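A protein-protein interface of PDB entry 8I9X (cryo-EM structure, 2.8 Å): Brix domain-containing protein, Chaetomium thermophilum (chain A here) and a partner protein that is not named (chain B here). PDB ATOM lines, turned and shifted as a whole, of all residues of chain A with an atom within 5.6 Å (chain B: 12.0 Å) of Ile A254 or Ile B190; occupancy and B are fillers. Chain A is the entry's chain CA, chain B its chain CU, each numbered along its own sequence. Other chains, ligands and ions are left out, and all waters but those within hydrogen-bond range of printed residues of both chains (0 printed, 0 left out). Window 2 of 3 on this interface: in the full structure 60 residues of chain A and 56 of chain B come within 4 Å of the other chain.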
ATOM      1  N   ILE A 244      21.101  35.839   9.024  1.00  0.00           N
ATOM      2  CA  ILE A 244      21.058  34.561   9.726  1.00  0.00           C
ATOM      3  C   ILE A 244      19.782  33.821   9.352  1.00  0.00           C
ATOM      4  O   ILE A 244      18.742  34.433   9.097  1.00  0.00           O
ATOM      5  CB  ILE A 244      21.146  34.736  11.259  1.00  0.00           C
ATOM      6  CG1 ILE A 244      20.032  35.658  11.764  1.00  0.00           C
ATOM      7  CG2 ILE A 244      22.523  35.218  11.677  1.00  0.00           C
ATOM      8  CD1 ILE A 244      19.802  35.583  13.251  1.00  0.00           C
ATOM      9  N   ILE A 245      19.879  32.495   9.307  1.00  0.00           N
ATOM     10  CA  ILE A 245      18.726  31.603   9.306  1.00  0.00           C
ATOM     11  C   ILE A 245      18.896  30.704  10.519  1.00  0.00           C
ATOM     12  O   ILE A 245      19.898  29.986  10.630  1.00  0.00           O
ATOM     13  CB  ILE A 245      18.620  30.776   8.019  1.00  0.00           C
ATOM     14  CG1 ILE A 245      18.458  31.691   6.808  1.00  0.00           C
ATOM     15  CG2 ILE A 245      17.457  29.801   8.107  1.00  0.00           C
ATOM     16  CD1 ILE A 245      18.305  30.947   5.512  1.00  0.00           C
ATOM     17  N   GLN A 246      17.934  30.743  11.429  1.00  0.00           N
ATOM     18  CA  GLN A 246      18.013  29.977  12.661  1.00  0.00           C
ATOM     19  C   GLN A 246      16.817  29.042  12.786  1.00  0.00           C
ATOM     20  O   GLN A 246      15.671  29.439  12.549  1.00  0.00           O
ATOM     21  CB  GLN A 246      18.134  30.912  13.872  1.00  0.00           C
ATOM     22  CG  GLN A 246      16.944  31.797  14.123  1.00  0.00           C
ATOM     23  CD  GLN A 246      17.147  32.742  15.290  1.00  0.00           C
ATOM     24  OE1 GLN A 246      18.177  32.706  15.962  1.00  0.00           O
ATOM     25  NE2 GLN A 246      16.167  33.604  15.527  1.00  0.00           N
ATOM     26  N   GLU A 247      17.102  27.792  13.136  1.00  0.00           N
ATOM     27  CA  GLU A 247      16.089  26.749  13.252  1.00  0.00           C
ATOM     28  C   GLU A 247      15.252  27.030  14.490  1.00  0.00           C
ATOM     29  O   GLU A 247      15.646  26.704  15.611  1.00  0.00           O
ATOM     30  CB  GLU A 247      16.743  25.375  13.329  1.00  0.00           C
ATOM     31  CG  GLU A 247      15.764  24.232  13.471  1.00  0.00           C
ATOM     32  CD  GLU A 247      16.392  23.002  14.089  1.00  0.00           C
ATOM     33  OE1 GLU A 247      17.323  23.153  14.906  1.00  0.00           O
ATOM     34  OE2 GLU A 247      15.962  21.882  13.746  1.00  0.00           O
ATOM     35  N   GLY A 252      16.576  29.291  18.638  1.00  0.00           N
ATOM     36  CA  GLY A 252      17.113  28.010  18.261  1.00  0.00           C
ATOM     37  C   GLY A 252      18.447  28.144  17.561  1.00  0.00           C
ATOM     38  O   GLY A 252      18.960  29.248  17.359  1.00  0.00           O
ATOM     39  N   PRO A 253      19.035  27.016  17.177  1.00  0.00           N
ATOM     40  CA  PRO A 253      20.351  27.049  16.537  1.00  0.00           C
ATOM     41  C   PRO A 253      20.304  27.751  15.191  1.00  0.00           C
ATOM     42  O   PRO A 253      19.294  27.748  14.486  1.00  0.00           O
ATOM     43  CB  PRO A 253      20.707  25.567  16.373  1.00  0.00           C
ATOM     44  CG  PRO A 253      19.824  24.855  17.335  1.00  0.00           C
ATOM     45  CD  PRO A 253      18.560  25.639  17.376  1.00  0.00           C
ATOM     46  N   ILE A 254      21.430  28.358  14.842  1.00  0.00           N
ATOM     47  CA  ILE A 254      21.586  29.047  13.570  1.00  0.00           C
ATOM     48  C   ILE A 254      21.975  28.036  12.501  1.00  0.00           C
ATOM     49  O   ILE A 254      22.929  27.269  12.675  1.00  0.00           O
ATOM     50  CB  ILE A 254      22.637  30.165  13.678  1.00  0.00           C
ATOM     51  CG1 ILE A 254      22.178  31.239  14.662  1.00  0.00           C
ATOM     52  CG2 ILE A 254      22.922  30.764  12.320  1.00  0.00           C
ATOM     53  CD1 ILE A 254      23.258  32.224  15.004  1.00  0.00           C
ATOM     54  N   LEU A 255      21.231  28.029  11.398  1.00  0.00           N
ATOM     55  CA  LEU A 255      21.529  27.172  10.259  1.00  0.00           C
ATOM     56  C   LEU A 255      22.360  27.856   9.188  1.00  0.00           C
ATOM     57  O   LEU A 255      22.976  27.171   8.370  1.00  0.00           O
ATOM     58  CB  LEU A 255      20.229  26.666   9.624  1.00  0.00           C
ATOM     59  CG  LEU A 255      19.266  25.948  10.566  1.00  0.00           C
ATOM     60  CD1 LEU A 255      18.039  25.474   9.810  1.00  0.00           C
ATOM     61  CD2 LEU A 255      19.967  24.785  11.239  1.00  0.00           C
ATOM     62  N   TYR A 256      22.389  29.185   9.177  1.00  0.00           N
ATOM     63  CA  TYR A 256      23.141  29.958   8.200  1.00  0.00           C
ATOM     64  C   TYR A 256      23.499  31.308   8.798  1.00  0.00           C
ATOM     65  O   TYR A 256      22.659  31.950   9.427  1.00  0.00           O
ATOM     66  CB  TYR A 256      22.340  30.163   6.911  1.00  0.00           C
ATOM     67  CG  TYR A 256      23.099  30.891   5.830  1.00  0.00           C
ATOM     68  CD1 TYR A 256      24.131  30.276   5.139  1.00  0.00           C
ATOM     69  CD2 TYR A 256      22.790  32.205   5.513  1.00  0.00           C
ATOM     70  CE1 TYR A 256      24.825  30.948   4.154  1.00  0.00           C
ATOM     71  CE2 TYR A 256      23.475  32.882   4.532  1.00  0.00           C
ATOM     72  CZ  TYR A 256      24.492  32.250   3.854  1.00  0.00           C
ATOM     73  OH  TYR A 256      25.182  32.925   2.875  1.00  0.00           O
ATOM     74  N   GLU A 257      24.744  31.733   8.598  1.00  0.00           N
ATOM     75  CA  GLU A 257      25.177  33.075   8.956  1.00  0.00           C
ATOM     76  C   GLU A 257      26.072  33.603   7.846  1.00  0.00           C
ATOM     77  O   GLU A 257      26.928  32.878   7.335  1.00  0.00           O
ATOM     78  CB  GLU A 257      25.905  33.098  10.308  1.00  0.00           C
ATOM     79  CG  GLU A 257      26.274  34.492  10.791  1.00  0.00           C
ATOM     80  CD  GLU A 257      27.466  34.495  11.726  1.00  0.00           C
ATOM     81  OE1 GLU A 257      27.306  34.077  12.891  1.00  0.00           O
ATOM     82  OE2 GLU A 257      28.558  34.917  11.303  1.00  0.00           O
ATOM     83  N   LYS A 259      28.592  35.730   7.290  1.00  0.00           N
ATOM     84  CA  LYS A 259      30.048  35.834   7.410  1.00  0.00           C
ATOM     85  C   LYS A 259      30.645  36.881   6.478  1.00  0.00           C
ATOM     86  O   LYS A 259      31.873  37.017   6.431  1.00  0.00           O
ATOM     87  CB  LYS A 259      30.762  34.496   7.155  1.00  0.00           C
ATOM     88  CG  LYS A 259      30.410  33.375   8.119  1.00  0.00           C
ATOM     89  CD  LYS A 259      30.802  33.738   9.539  1.00  0.00           C
ATOM     90  CE  LYS A 259      32.312  33.830   9.676  1.00  0.00           C
ATOM     91  NZ  LYS A 259      32.965  32.515   9.451  1.00  0.00           N
ATOM     92  N   ILE B 190      29.244  29.339   8.854  1.00  0.00           N
ATOM     93  CA  ILE B 190      28.152  28.472   9.274  1.00  0.00           C
ATOM     94  C   ILE B 190      27.135  28.308   8.153  1.00  0.00           C
ATOM     95  O   ILE B 190      26.364  29.219   7.863  1.00  0.00           O
ATOM     96  CB  ILE B 190      27.470  29.006  10.544  1.00  0.00           C
ATOM     97  CG1 ILE B 190      28.454  29.025  11.713  1.00  0.00           C
ATOM     98  CG2 ILE B 190      26.265  28.154  10.900  1.00  0.00           C
ATOM     99  CD1 ILE B 190      27.942  29.772  12.925  1.00  0.00           C
ATOM    100  N   ASN B 191      27.144  27.135   7.517  1.00  0.00           N
ATOM    101  CA  ASN B 191      26.161  26.768   6.507  1.00  0.00           C
ATOM    102  C   ASN B 191      25.765  25.312   6.762  1.00  0.00           C
ATOM    103  O   ASN B 191      26.344  24.365   6.234  1.00  0.00           O
ATOM    104  CB  ASN B 191      26.701  26.964   5.090  1.00  0.00           C
ATOM    105  CG  ASN B 191      25.601  27.082   4.059  1.00  0.00           C
ATOM    106  OD1 ASN B 191      24.451  26.730   4.318  1.00  0.00           O
ATOM    107  ND2 ASN B 191      25.949  27.575   2.877  1.00  0.00           N
ATOM    108  N   ASN B 192      24.743  25.124   7.593  1.00  0.00           N
ATOM    109  CA  ASN B 192      24.271  23.783   7.907  1.00  0.00           C
ATOM    110  C   ASN B 192      23.251  23.340   6.869  1.00  0.00           C
ATOM    111  O   ASN B 192      22.051  23.580   7.028  1.00  0.00           O
ATOM    112  CB  ASN B 192      23.671  23.736   9.312  1.00  0.00           C
ATOM    113  CG  ASN B 192      23.357  22.323   9.762  1.00  0.00           C
ATOM    114  OD1 ASN B 192      23.959  21.362   9.289  1.00  0.00           O
ATOM    115  ND2 ASN B 192      22.416  22.196  10.688  1.00  0.00           N
ATOM    116  N   LYS B 193      23.724  22.696   5.801  1.00  0.00           N
ATOM    117  CA  LYS B 193      22.836  22.341   4.700  1.00  0.00           C
ATOM    118  C   LYS B 193      21.845  21.258   5.108  1.00  0.00           C
ATOM    119  O   LYS B 193      20.681  21.288   4.695  1.00  0.00           O
ATOM    120  CB  LYS B 193      23.657  21.906   3.488  1.00  0.00           C
ATOM    121  CG  LYS B 193      24.463  23.037   2.869  1.00  0.00           C
ATOM    122  CD  LYS B 193      25.270  22.558   1.677  1.00  0.00           C
ATOM    123  CE  LYS B 193      26.150  23.666   1.128  1.00  0.00           C
ATOM    124  NZ  LYS B 193      26.985  23.200  -0.013  1.00  0.00           N
ATOM    125  N   GLU B 194      22.283  20.299   5.926  1.00  0.00           N
ATOM    126  CA  GLU B 194      21.372  19.259   6.392  1.00  0.00           C
ATOM    127  C   GLU B 194      20.248  19.845   7.239  1.00  0.00           C
ATOM    128  O   GLU B 194      19.077  19.490   7.065  1.00  0.00           O
ATOM    129  CB  GLU B 194      22.144  18.196   7.173  1.00  0.00           C
ATOM    130  CG  GLU B 194      23.090  17.360   6.323  1.00  0.00           C
ATOM    131  CD  GLU B 194      24.473  17.970   6.206  1.00  0.00           C
ATOM    132  OE1 GLU B 194      24.713  19.026   6.827  1.00  0.00           O
ATOM    133  OE2 GLU B 194      25.319  17.392   5.492  1.00  0.00           O
ATOM    134  N   GLY B 195      20.584  20.744   8.168  1.00  0.00           N
ATOM    135  CA  GLY B 195      19.555  21.384   8.968  1.00  0.00           C
ATOM    136  C   GLY B 195      18.652  22.285   8.154  1.00  0.00           C
ATOM    137  O   GLY B 195      17.439  22.334   8.390  1.00  0.00           O
ATOM    138  N   LEU B 196      19.223  23.002   7.184  1.00  0.00           N
ATOM    139  CA  LEU B 196      18.420  23.825   6.290  1.00  0.00           C
ATOM    140  C   LEU B 196      17.411  22.974   5.533  1.00  0.00           C
ATOM    141  O   LEU B 196      16.232  23.332   5.446  1.00  0.00           O
ATOM    142  CB  LEU B 196      19.334  24.573   5.320  1.00  0.00           C
ATOM    143  CG  LEU B 196      19.991  25.859   5.826  1.00  0.00           C
ATOM    144  CD1 LEU B 196      21.145  26.260   4.923  1.00  0.00           C
ATOM    145  CD2 LEU B 196      18.980  26.987   5.929  1.00  0.00           C
ATOM    146  N   LEU B 197      17.848  21.826   5.011  1.00  0.00           N
ATOM    147  CA  LEU B 197      16.939  20.928   4.310  1.00  0.00           C
ATOM    148  C   LEU B 197      15.904  20.304   5.237  1.00  0.00           C
ATOM    149  O   LEU B 197      14.761  20.104   4.824  1.00  0.00           O
ATOM    150  CB  LEU B 197      17.727  19.830   3.595  1.00  0.00           C
ATOM    151  CG  LEU B 197      18.565  20.264   2.392  1.00  0.00           C
ATOM    152  CD1 LEU B 197      19.351  19.091   1.828  1.00  0.00           C
ATOM    153  CD2 LEU B 197      17.687  20.884   1.317  1.00  0.00           C
ATOM    154  N   THR B 198      16.278  19.970   6.472  1.00  0.00           N
ATOM    155  CA  THR B 198      15.299  19.434   7.412  1.00  0.00           C
ATOM    156  C   THR B 198      14.204  20.452   7.702  1.00  0.00           C
ATOM    157  O   THR B 198      13.006  20.127   7.680  1.00  0.00           O
ATOM    158  CB  THR B 198      15.998  19.018   8.706  1.00  0.00           C
ATOM    159  OG1 THR B 198      17.127  18.196   8.391  1.00  0.00           O
ATOM    160  CG2 THR B 198      15.047  18.242   9.606  1.00  0.00           C
ATOM    161  N   ALA B 199      14.600  21.700   7.962  1.00  0.00           N
ATOM    162  CA  ALA B 199      13.622  22.761   8.182  1.00  0.00           C
ATOM    163  C   ALA B 199      12.777  22.982   6.934  1.00  0.00           C
ATOM    164  O   ALA B 199      11.563  23.213   7.018  1.00  0.00           O
ATOM    165  CB  ALA B 199      14.332  24.050   8.596  1.00  0.00           C
ATOM    166  N   ARG B 202       9.967  20.409   6.737  1.00  0.00           N
ATOM    167  CA  ARG B 202       8.949  20.552   7.740  1.00  0.00           C
ATOM    168  C   ARG B 202       7.931  21.579   7.368  1.00  0.00           C
ATOM    169  O   ARG B 202       6.913  21.385   7.869  1.00  0.00           O
ATOM    170  CB  ARG B 202       9.539  20.752   9.131  1.00  0.00           C
ATOM    171  CG  ARG B 202      10.590  19.799   9.647  1.00  0.00           C
ATOM    172  CD  ARG B 202      10.694  20.029  11.143  1.00  0.00           C
ATOM    173  NE  ARG B 202      11.697  20.998  11.434  1.00  0.00           N
ATOM    174  CZ  ARG B 202      12.882  20.759  11.946  1.00  0.00           C
ATOM    175  NH1 ARG B 202      13.224  19.550  12.308  1.00  0.00           N
ATOM    176  NH2 ARG B 202      13.743  21.738  12.091  1.00  0.00           N
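No residue of chain B comes within 4 Å of Ile A244. Printed residues of chain B within 4 Å of Glu A247: Arg B202. No residue of chain B comes within 4 Å of Gly A252. No residue of chain B comes within 4 Å of Pro A253. Printed residues of chain B within 4 Å of Leu A255: Ile B190 (3.99 Å), Asn B191 (3.7 Å), Asn B192 (2.8 Å), Gly B195 (3.5 Å) and Leu B196 (3.8 Å). Of chain B, only Ile B190 (3.3 Å) and Asn B191 (3.7 Å) come within 4 Å of Tyr A256. Printed residues of chain A within 4 Å of Ile B190: Ile A254 (3.9 Å), Leu A255 (3.99 Å), Tyr A256 (3.3 Å) and Glu A257 (3.1 Å). Glu B194 touches none of the printed residues of chain A. Printed residues of chain A within 4 Å of Gly B195: Leu A255 (3.5 Å). Leu B197 touches none of the printed residues of chain A. The nearest printed residue of chain A that does not touch Leu B196 is Tyr A256 (4.5 Å).
The side-chain amide oxygen (OD1) of Asn B192 lies close to the side-chain carboxylate (OE1) of Glu B194 (3.5 Å). The side-chain amide nitrogen (ND2) of Asn B192 sits close to the backbone NH (N) of Gly B195 (3.4 Å). O of Ile A245 sits at hydrogen-bond distance from N of Leu A255, 2.5 Å away. N of Ile A245 lies within hydrogen-bond range of O of Tyr A256. O of Pro A253 is in hydrogen-bond range of N of Glu A247.
The backbone carbonyl oxygen (O) of Ile B190 sits at hydrogen-bond distance from the backbone NH (N) of Glu A257, at 3.1 Å. The backbone NH (N) of Asn B192 is in hydrogen-bond range of the backbone carbonyl oxygen (O) of Leu A255 (2.8 Å). OE2 of Glu A247 is in salt-bridge range of NH2 of Arg B202.
Printed residues of chain B that touch a printed residue of chain A: Ile B190, Asn B191, Asn B192, Gly B195, Leu B196 and Arg B202. Hydrophobic or aromatic side chains of chain A within 4 Å of the printed part of chain B: Ile A245, Leu A255 and Tyr A256. Along chain A the printed residues that touch a printed residue of chain B span positions 245 to 257. Among the printed residues, Asp or Glu carboxylates within 4 Å of a Lys or Arg side-chain nitrogen of the other chain: Glu A247 with Arg B202.
Ile A245 touches Leu B196 (CG2 to CD2, 3.9 Å). Ile B190 touches Ile A254. O of Leu A255 touches O of Ile B190, at 3.99 Å. CA of Asn B191 touches O of Leu A255, 3.7 Å away. CD1 of Leu A255 touches O of Gly B195 (3.5 Å). Leu B196 touches Leu A255 (N to CD1, 3.8 Å). Tyr A256 touches Ile B190 (CA to O, 3.3 Å). CD1 of Tyr A256 touches OD1 of Asn B191 (3.7 Å).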
